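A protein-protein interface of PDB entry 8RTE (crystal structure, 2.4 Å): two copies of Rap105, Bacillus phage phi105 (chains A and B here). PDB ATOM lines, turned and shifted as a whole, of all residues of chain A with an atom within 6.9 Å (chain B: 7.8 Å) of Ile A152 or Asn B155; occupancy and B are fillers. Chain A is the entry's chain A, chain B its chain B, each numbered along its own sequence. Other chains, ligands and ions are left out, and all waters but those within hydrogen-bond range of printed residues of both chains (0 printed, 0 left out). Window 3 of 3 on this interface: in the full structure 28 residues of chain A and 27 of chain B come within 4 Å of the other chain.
The backbone carbonyl oxygen (O) of Tyr A144 sits at hydrogen-bond distance from the backbone NH (N) of Gln A149 (2.7 Å).
Gln A149 touches Leu B151, and with the chains exchanged Leu A151 touches Gln B149. Leu A151 touches Ile B152, and with the chains exchanged Ile A152 touches Leu B151. Ile A152 touches its own counterpart, Ile B152. Ile A152 touches Asn B155, and with the chains exchanged Asn A155 touches Ile B152. Positions printed for both chains: 141, 149, 150, 151, 152, 153, 154, 155, 156, 157 and 184.
Of chain B, only Leu B151 (3.6 Å), Ile B152 (3.6 Å) and Asn B155 (3.6 Å) come within 4 Å of Ile A152. Asn B155 touches one residue of chain A. Printed residues of chain A within 4 Å of Gln B149: Leu A151. Of the printed residues of chain B, Gln A149 touches Leu B151 (3.6 Å). Asn B184 touches none of the printed residues of chain A. Ser B160 touches none of the printed residues of chain A. The nearest residue of chain B that does not touch Ile A152 is Gln B149 (6.2 Å). The nearest residue of chain A that does not touch Asn B155 is Tyr A156 (5.4 Å).
Along chain B the printed residues that touch a printed residue of chain A span positions 149 to 155.
Among the printed residues, merely in contact across the chains: Tyr A144 with Leu B151 (3.5 Å), Asn A155 with Ile B152 (3.5 Å), Leu A151 with Gln B149 (3.5 Å), Ile A152 with Leu B151 (3.6 Å), Ile A152 with Asn B155 (3.6 Å), Ile A152 with Ile B152 (3.6 Å), Gln A149 with Leu B151 (3.6 Å) and Leu A151 with Ile B152 (3.7 Å).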
ATOM      1  N   VAL A 140      -1.183   5.280  31.752  1.00  0.00           N
ATOM      2  CA  VAL A 140      -0.641   6.624  31.578  1.00  0.00           C
ATOM      3  C   VAL A 140      -1.181   7.248  30.299  1.00  0.00           C
ATOM      4  O   VAL A 140      -1.561   8.424  30.276  1.00  0.00           O
ATOM      5  CB  VAL A 140       0.900   6.581  31.583  1.00  0.00           C
ATOM      6  CG1 VAL A 140       1.474   7.886  31.060  1.00  0.00           C
ATOM      7  CG2 VAL A 140       1.412   6.306  32.975  1.00  0.00           C
ATOM      8  N   ALA A 141      -1.231   6.464  29.218  1.00  0.00           N
ATOM      9  CA  ALA A 141      -1.731   6.977  27.948  1.00  0.00           C
ATOM     10  C   ALA A 141      -3.190   7.393  28.056  1.00  0.00           C
ATOM     11  O   ALA A 141      -3.598   8.409  27.482  1.00  0.00           O
ATOM     12  CB  ALA A 141      -1.553   5.928  26.852  1.00  0.00           C
ATOM     13  N   TYR A 144      -3.377  10.862  29.832  1.00  0.00           N
ATOM     14  CA  TYR A 144      -2.972  11.969  28.978  1.00  0.00           C
ATOM     15  C   TYR A 144      -4.014  12.237  27.896  1.00  0.00           C
ATOM     16  O   TYR A 144      -4.216  13.385  27.478  1.00  0.00           O
ATOM     17  CB  TYR A 144      -1.607  11.677  28.370  1.00  0.00           C
ATOM     18  CG  TYR A 144      -0.475  12.031  29.298  1.00  0.00           C
ATOM     19  CD1 TYR A 144      -0.275  13.341  29.703  1.00  0.00           C
ATOM     20  CD2 TYR A 144       0.396  11.056  29.769  1.00  0.00           C
ATOM     21  CE1 TYR A 144       0.757  13.678  30.555  1.00  0.00           C
ATOM     22  CE2 TYR A 144       1.440  11.384  30.619  1.00  0.00           C
ATOM     23  CZ  TYR A 144       1.612  12.700  31.006  1.00  0.00           C
ATOM     24  OH  TYR A 144       2.636  13.065  31.848  1.00  0.00           O
ATOM     25  N   MET A 145      -4.690  11.201  27.416  1.00  0.00           N
ATOM     26  CA  MET A 145      -5.761  11.424  26.422  1.00  0.00           C
ATOM     27  C   MET A 145      -6.905  12.210  27.077  1.00  0.00           C
ATOM     28  O   MET A 145      -7.472  13.075  26.412  1.00  0.00           O
ATOM     29  CB  MET A 145      -6.241  10.085  25.861  1.00  0.00           C
ATOM     30  CG  MET A 145      -7.601  10.119  25.218  1.00  0.00           C
ATOM     31  SD  MET A 145      -8.664   8.862  25.929  1.00  0.00           S
ATOM     32  CE  MET A 145      -9.451   9.776  27.251  1.00  0.00           C
ATOM     33  N   GLN A 149      -3.739  15.497  25.794  1.00  0.00           N
ATOM     34  CA  GLN A 149      -2.293  15.455  25.577  1.00  0.00           C
ATOM     35  C   GLN A 149      -2.028  14.319  24.599  1.00  0.00           C
ATOM     36  O   GLN A 149      -1.596  13.225  24.963  1.00  0.00           O
ATOM     37  CB  GLN A 149      -1.550  15.250  26.894  1.00  0.00           C
ATOM     38  CG  GLN A 149      -1.806  16.317  27.949  1.00  0.00           C
ATOM     39  CD  GLN A 149      -0.922  17.536  27.793  1.00  0.00           C
ATOM     40  OE1 GLN A 149      -0.085  17.599  26.895  1.00  0.00           O
ATOM     41  NE2 GLN A 149      -1.118  18.525  28.660  1.00  0.00           N
ATOM     42  N   SER A 150      -2.278  14.609  23.322  1.00  0.00           N
ATOM     43  CA  SER A 150      -2.458  13.553  22.337  1.00  0.00           C
ATOM     44  C   SER A 150      -1.139  12.889  21.956  1.00  0.00           C
ATOM     45  O   SER A 150      -1.057  11.659  21.898  1.00  0.00           O
ATOM     46  CB  SER A 150      -3.162  14.120  21.106  1.00  0.00           C
ATOM     47  OG  SER A 150      -4.375  14.761  21.470  1.00  0.00           O
ATOM     48  N   LEU A 151      -0.094  13.678  21.697  1.00  0.00           N
ATOM     49  CA  LEU A 151       1.169  13.098  21.250  1.00  0.00           C
ATOM     50  C   LEU A 151       1.819  12.264  22.349  1.00  0.00           C
ATOM     51  O   LEU A 151       2.310  11.158  22.093  1.00  0.00           O
ATOM     52  CB  LEU A 151       2.110  14.199  20.774  1.00  0.00           C
ATOM     53  CG  LEU A 151       1.647  14.908  19.498  1.00  0.00           C
ATOM     54  CD1 LEU A 151       2.712  15.869  19.002  1.00  0.00           C
ATOM     55  CD2 LEU A 151       1.255  13.915  18.404  1.00  0.00           C
ATOM     56  N   ILE A 152       1.840  12.782  23.579  1.00  0.00           N
ATOM     57  CA  ILE A 152       2.371  12.019  24.707  1.00  0.00           C
ATOM     58  C   ILE A 152       1.584  10.729  24.895  1.00  0.00           C
ATOM     59  O   ILE A 152       2.155   9.650  25.100  1.00  0.00           O
ATOM     60  CB  ILE A 152       2.367  12.879  25.984  1.00  0.00           C
ATOM     61  CG1 ILE A 152       3.356  14.033  25.847  1.00  0.00           C
ATOM     62  CG2 ILE A 152       2.710  12.041  27.203  1.00  0.00           C
ATOM     63  CD1 ILE A 152       4.803  13.628  26.091  1.00  0.00           C
ATOM     64  N   SER A 153       0.256  10.825  24.841  1.00  0.00           N
ATOM     65  CA  SER A 153      -0.574   9.633  24.979  1.00  0.00           C
ATOM     66  C   SER A 153      -0.274   8.620  23.879  1.00  0.00           C
ATOM     67  O   SER A 153      -0.266   7.408  24.127  1.00  0.00           O
ATOM     68  CB  SER A 153      -2.051  10.018  24.964  1.00  0.00           C
ATOM     69  OG  SER A 153      -2.857   8.869  25.168  1.00  0.00           O
ATOM     70  N   LEU A 154      -0.025   9.096  22.657  1.00  0.00           N
ATOM     71  CA  LEU A 154       0.244   8.180  21.554  1.00  0.00           C
ATOM     72  C   LEU A 154       1.575   7.461  21.745  1.00  0.00           C
ATOM     73  O   LEU A 154       1.671   6.253  21.499  1.00  0.00           O
ATOM     74  CB  LEU A 154       0.224   8.933  20.228  1.00  0.00           C
ATOM     75  CG  LEU A 154      -1.158   9.147  19.613  1.00  0.00           C
ATOM     76  CD1 LEU A 154      -1.059  10.119  18.450  1.00  0.00           C
ATOM     77  CD2 LEU A 154      -1.752   7.823  19.162  1.00  0.00           C
ATOM     78  N   ASN A 155       2.615   8.186  22.173  1.00  0.00           N
ATOM     79  CA  ASN A 155       3.906   7.553  22.434  1.00  0.00           C
ATOM     80  C   ASN A 155       3.770   6.416  23.439  1.00  0.00           C
ATOM     81  O   ASN A 155       4.338   5.336  23.247  1.00  0.00           O
ATOM     82  CB  ASN A 155       4.901   8.593  22.955  1.00  0.00           C
ATOM     83  CG  ASN A 155       5.432   9.509  21.864  1.00  0.00           C
ATOM     84  OD1 ASN A 155       5.169   9.306  20.677  1.00  0.00           O
ATOM     85  ND2 ASN A 155       6.180  10.531  22.269  1.00  0.00           N
ATOM     86  N   TYR A 156       3.012   6.640  24.515  1.00  0.00           N
ATOM     87  CA  TYR A 156       2.818   5.609  25.527  1.00  0.00           C
ATOM     88  C   TYR A 156       2.028   4.429  24.974  1.00  0.00           C
ATOM     89  O   TYR A 156       2.466   3.278  25.068  1.00  0.00           O
ATOM     90  CB  TYR A 156       2.120   6.205  26.747  1.00  0.00           C
ATOM     91  CG  TYR A 156       3.058   6.941  27.671  1.00  0.00           C
ATOM     92  CD1 TYR A 156       4.008   6.262  28.418  1.00  0.00           C
ATOM     93  CD2 TYR A 156       2.992   8.323  27.795  1.00  0.00           C
ATOM     94  CE1 TYR A 156       4.870   6.936  29.261  1.00  0.00           C
ATOM     95  CE2 TYR A 156       3.848   9.006  28.635  1.00  0.00           C
ATOM     96  CZ  TYR A 156       4.785   8.308  29.365  1.00  0.00           C
ATOM     97  OH  TYR A 156       5.639   8.988  30.202  1.00  0.00           O
ATOM     98  N   ILE A 157       0.849   4.696  24.404  1.00  0.00           N
ATOM     99  CA  ILE A 157      -0.034   3.611  23.981  1.00  0.00           C
ATOM    100  C   ILE A 157       0.568   2.810  22.830  1.00  0.00           C
ATOM    101  O   ILE A 157       0.337   1.599  22.727  1.00  0.00           O
ATOM    102  CB  ILE A 157      -1.427   4.164  23.623  1.00  0.00           C
ATOM    103  CG1 ILE A 157      -2.467   3.041  23.657  1.00  0.00           C
ATOM    104  CG2 ILE A 157      -1.408   4.888  22.274  1.00  0.00           C
ATOM    105  CD1 ILE A 157      -2.566   2.362  25.018  1.00  0.00           C
ATOM    106  N   ASN A 184      -7.108   9.948  20.495  1.00  0.00           N
ATOM    107  CA  ASN A 184      -5.982  10.852  20.272  1.00  0.00           C
ATOM    108  C   ASN A 184      -6.004  11.432  18.864  1.00  0.00           C
ATOM    109  O   ASN A 184      -5.762  12.631  18.676  1.00  0.00           O
ATOM    110  CB  ASN A 184      -4.660  10.136  20.531  1.00  0.00           C
ATOM    111  CG  ASN A 184      -4.408   9.907  22.003  1.00  0.00           C
ATOM    112  OD1 ASN A 184      -4.791  10.725  22.839  1.00  0.00           O
ATOM    113  ND2 ASN A 184      -3.766   8.793  22.331  1.00  0.00           N
ATOM    114  N   TYR B 137      18.037  16.385  19.684  1.00  0.00           N
ATOM    115  CA  TYR B 137      16.922  16.537  20.617  1.00  0.00           C
ATOM    116  C   TYR B 137      16.595  18.003  20.877  1.00  0.00           C
ATOM    117  O   TYR B 137      15.424  18.369  21.026  1.00  0.00           O
ATOM    118  CB  TYR B 137      17.234  15.818  21.931  1.00  0.00           C
ATOM    119  CG  TYR B 137      17.443  14.324  21.796  1.00  0.00           C
ATOM    120  CD1 TYR B 137      16.843  13.609  20.768  1.00  0.00           C
ATOM    121  CD2 TYR B 137      18.241  13.629  22.700  1.00  0.00           C
ATOM    122  CE1 TYR B 137      17.033  12.240  20.638  1.00  0.00           C
ATOM    123  CE2 TYR B 137      18.439  12.262  22.580  1.00  0.00           C
ATOM    124  CZ  TYR B 137      17.834  11.572  21.548  1.00  0.00           C
ATOM    125  OH  TYR B 137      18.025  10.211  21.425  1.00  0.00           O
ATOM    126  N   ALA B 141      13.057  19.585  20.076  1.00  0.00           N
ATOM    127  CA  ALA B 141      12.356  20.217  21.187  1.00  0.00           C
ATOM    128  C   ALA B 141      11.977  21.652  20.855  1.00  0.00           C
ATOM    129  O   ALA B 141      10.896  22.119  21.233  1.00  0.00           O
ATOM    130  CB  ALA B 141      13.214  20.172  22.449  1.00  0.00           C
ATOM    131  N   GLN B 149       3.673  22.248  21.877  1.00  0.00           N
ATOM    132  CA  GLN B 149       3.670  20.841  22.268  1.00  0.00           C
ATOM    133  C   GLN B 149       4.693  20.692  23.389  1.00  0.00           C
ATOM    134  O   GLN B 149       5.827  20.252  23.195  1.00  0.00           O
ATOM    135  CB  GLN B 149       3.970  19.945  21.073  1.00  0.00           C
ATOM    136  CG  GLN B 149       2.958  20.082  19.944  1.00  0.00           C
ATOM    137  CD  GLN B 149       1.740  19.209  20.161  1.00  0.00           C
ATOM    138  OE1 GLN B 149       1.656  18.485  21.154  1.00  0.00           O
ATOM    139  NE2 GLN B 149       0.783  19.280  19.241  1.00  0.00           N
ATOM    140  N   SER B 150       4.263  21.078  24.593  1.00  0.00           N
ATOM    141  CA  SER B 150       5.191  21.371  25.680  1.00  0.00           C
ATOM    142  C   SER B 150       5.782  20.104  26.292  1.00  0.00           C
ATOM    143  O   SER B 150       6.994  20.036  26.527  1.00  0.00           O
ATOM    144  CB  SER B 150       4.476  22.211  26.736  1.00  0.00           C
ATOM    145  OG  SER B 150       3.903  23.359  26.132  1.00  0.00           O
ATOM    146  N   LEU B 151       4.950  19.097  26.566  1.00  0.00           N
ATOM    147  CA  LEU B 151       5.460  17.876  27.191  1.00  0.00           C
ATOM    148  C   LEU B 151       6.408  17.127  26.263  1.00  0.00           C
ATOM    149  O   LEU B 151       7.449  16.624  26.706  1.00  0.00           O
ATOM    150  CB  LEU B 151       4.306  16.973  27.618  1.00  0.00           C
ATOM    151  CG  LEU B 151       3.445  17.424  28.796  1.00  0.00           C
ATOM    152  CD1 LEU B 151       2.457  16.331  29.134  1.00  0.00           C
ATOM    153  CD2 LEU B 151       4.317  17.742  30.004  1.00  0.00           C
ATOM    154  N   ILE B 152       6.053  17.017  24.982  1.00  0.00           N
ATOM    155  CA  ILE B 152       6.948  16.394  24.010  1.00  0.00           C
ATOM    156  C   ILE B 152       8.268  17.154  23.956  1.00  0.00           C
ATOM    157  O   ILE B 152       9.355  16.561  23.997  1.00  0.00           O
ATOM    158  CB  ILE B 152       6.277  16.339  22.624  1.00  0.00           C
ATOM    159  CG1 ILE B 152       5.051  15.419  22.653  1.00  0.00           C
ATOM    160  CG2 ILE B 152       7.266  15.890  21.552  1.00  0.00           C
ATOM    161  CD1 ILE B 152       5.378  13.941  22.579  1.00  0.00           C
ATOM    162  N   SER B 153       8.190  18.486  23.888  1.00  0.00           N
ATOM    163  CA  SER B 153       9.398  19.304  23.854  1.00  0.00           C
ATOM    164  C   SER B 153      10.242  19.111  25.108  1.00  0.00           C
ATOM    165  O   SER B 153      11.475  19.079  25.034  1.00  0.00           O
ATOM    166  CB  SER B 153       9.028  20.774  23.676  1.00  0.00           C
ATOM    167  OG  SER B 153      10.201  21.567  23.581  1.00  0.00           O
ATOM    168  N   LEU B 154       9.595  18.985  26.272  1.00  0.00           N
ATOM    169  CA  LEU B 154      10.342  18.826  27.516  1.00  0.00           C
ATOM    170  C   LEU B 154      11.058  17.485  27.580  1.00  0.00           C
ATOM    171  O   LEU B 154      12.216  17.419  28.010  1.00  0.00           O
ATOM    172  CB  LEU B 154       9.415  18.980  28.721  1.00  0.00           C
ATOM    173  CG  LEU B 154       9.168  20.409  29.189  1.00  0.00           C
ATOM    174  CD1 LEU B 154       8.057  20.442  30.225  1.00  0.00           C
ATOM    175  CD2 LEU B 154      10.460  20.999  29.740  1.00  0.00           C
ATOM    176  N   ASN B 155      10.382  16.404  27.182  1.00  0.00           N
ATOM    177  CA  ASN B 155      11.029  15.095  27.177  1.00  0.00           C
ATOM    178  C   ASN B 155      12.291  15.112  26.326  1.00  0.00           C
ATOM    179  O   ASN B 155      13.322  14.559  26.724  1.00  0.00           O
ATOM    180  CB  ASN B 155      10.050  14.027  26.691  1.00  0.00           C
ATOM    181  CG  ASN B 155       9.027  13.655  27.744  1.00  0.00           C
ATOM    182  OD1 ASN B 155       9.114  14.090  28.892  1.00  0.00           O
ATOM    183  ND2 ASN B 155       8.044  12.852  27.355  1.00  0.00           N
ATOM    184  N   TYR B 156      12.230  15.749  25.155  1.00  0.00           N
ATOM    185  CA  TYR B 156      13.410  15.873  24.309  1.00  0.00           C
ATOM    186  C   TYR B 156      14.469  16.740  24.976  1.00  0.00           C
ATOM    187  O   TYR B 156      15.622  16.319  25.142  1.00  0.00           O
ATOM    188  CB  TYR B 156      13.025  16.459  22.948  1.00  0.00           C
ATOM    189  CG  TYR B 156      12.536  15.448  21.934  1.00  0.00           C
ATOM    190  CD1 TYR B 156      13.412  14.525  21.376  1.00  0.00           C
ATOM    191  CD2 TYR B 156      11.213  15.432  21.516  1.00  0.00           C
ATOM    192  CE1 TYR B 156      12.979  13.605  20.440  1.00  0.00           C
ATOM    193  CE2 TYR B 156      10.769  14.510  20.579  1.00  0.00           C
ATOM    194  CZ  TYR B 156      11.662  13.602  20.044  1.00  0.00           C
ATOM    195  OH  TYR B 156      11.235  12.682  19.113  1.00  0.00           O
ATOM    196  N   ILE B 157      14.094  17.960  25.371  1.00  0.00           N
ATOM    197  CA  ILE B 157      15.079  18.906  25.887  1.00  0.00           C
ATOM    198  C   ILE B 157      15.682  18.405  27.195  1.00  0.00           C
ATOM    199  O   ILE B 157      16.851  18.687  27.490  1.00  0.00           O
ATOM    200  CB  ILE B 157      14.453  20.309  26.017  1.00  0.00           C
ATOM    201  CG1 ILE B 157      15.539  21.390  26.083  1.00  0.00           C
ATOM    202  CG2 ILE B 157      13.546  20.399  27.217  1.00  0.00           C
ATOM    203  CD1 ILE B 157      16.442  21.418  24.871  1.00  0.00           C
ATOM    204  N   ASN B 158      14.916  17.652  27.998  1.00  0.00           N
ATOM    205  CA  ASN B 158      15.464  17.131  29.246  1.00  0.00           C
ATOM    206  C   ASN B 158      16.624  16.182  28.990  1.00  0.00           C
ATOM    207  O   ASN B 158      17.569  16.132  29.784  1.00  0.00           O
ATOM    208  CB  ASN B 158      14.372  16.442  30.059  1.00  0.00           C
ATOM    209  CG  ASN B 158      13.490  17.426  30.804  1.00  0.00           C
ATOM    210  OD1 ASN B 158      13.961  18.464  31.264  1.00  0.00           O
ATOM    211  ND2 ASN B 158      12.199  17.120  30.899  1.00  0.00           N
ATOM    212  N   ASP B 159      16.583  15.442  27.880  1.00  0.00           N
ATOM    213  CA  ASP B 159      17.722  14.612  27.511  1.00  0.00           C
ATOM    214  C   ASP B 159      18.908  15.472  27.093  1.00  0.00           C
ATOM    215  O   ASP B 159      20.050  15.179  27.467  1.00  0.00           O
ATOM    216  CB  ASP B 159      17.330  13.642  26.396  1.00  0.00           C
ATOM    217  CG  ASP B 159      16.571  12.426  26.913  1.00  0.00           C
ATOM    218  OD1 ASP B 159      16.630  12.157  28.134  1.00  0.00           O
ATOM    219  OD2 ASP B 159      15.926  11.729  26.098  1.00  0.00           O
ATOM    220  N   SER B 160      18.661  16.534  26.318  1.00  0.00           N
ATOM    221  CA  SER B 160      19.741  17.438  25.924  1.00  0.00           C
ATOM    222  C   SER B 160      20.418  18.073  27.135  1.00  0.00           C
ATOM    223  O   SER B 160      21.650  18.169  27.185  1.00  0.00           O
ATOM    224  CB  SER B 160      19.210  18.522  24.988  1.00  0.00           C
ATOM    225  OG  SER B 160      18.932  17.998  23.703  1.00  0.00           O
ATOM    226  N   ILE B 161      19.630  18.507  28.123  1.00  0.00           N
ATOM    227  CA  ILE B 161      20.193  19.186  29.288  1.00  0.00           C
ATOM    228  C   ILE B 161      21.058  18.234  30.106  1.00  0.00           C
ATOM    229  O   ILE B 161      22.137  18.610  30.584  1.00  0.00           O
ATOM    230  CB  ILE B 161      19.066  19.814  30.130  1.00  0.00           C
ATOM    231  CG1 ILE B 161      18.585  21.101  29.470  1.00  0.00           C
ATOM    232  CG2 ILE B 161      19.527  20.099  31.553  1.00  0.00           C
ATOM    233  CD1 ILE B 161      17.304  21.607  30.041  1.00  0.00           C
ATOM    234  N   ASN B 184       8.419  26.010  27.650  1.00  0.00           N
ATOM    235  CA  ASN B 184       7.568  24.839  27.841  1.00  0.00           C
ATOM    236  C   ASN B 184       6.829  24.923  29.171  1.00  0.00           C
ATOM    237  O   ASN B 184       5.631  24.623  29.246  1.00  0.00           O
ATOM    238  CB  ASN B 184       8.399  23.560  27.768  1.00  0.00           C
ATOM    239  CG  ASN B 184       8.850  23.242  26.348  1.00  0.00           C
ATOM    240  OD1 ASN B 184       8.135  23.505  25.379  1.00  0.00           O
ATOM    241  ND2 ASN B 184      10.046  22.679  26.219  1.00  0.00           N
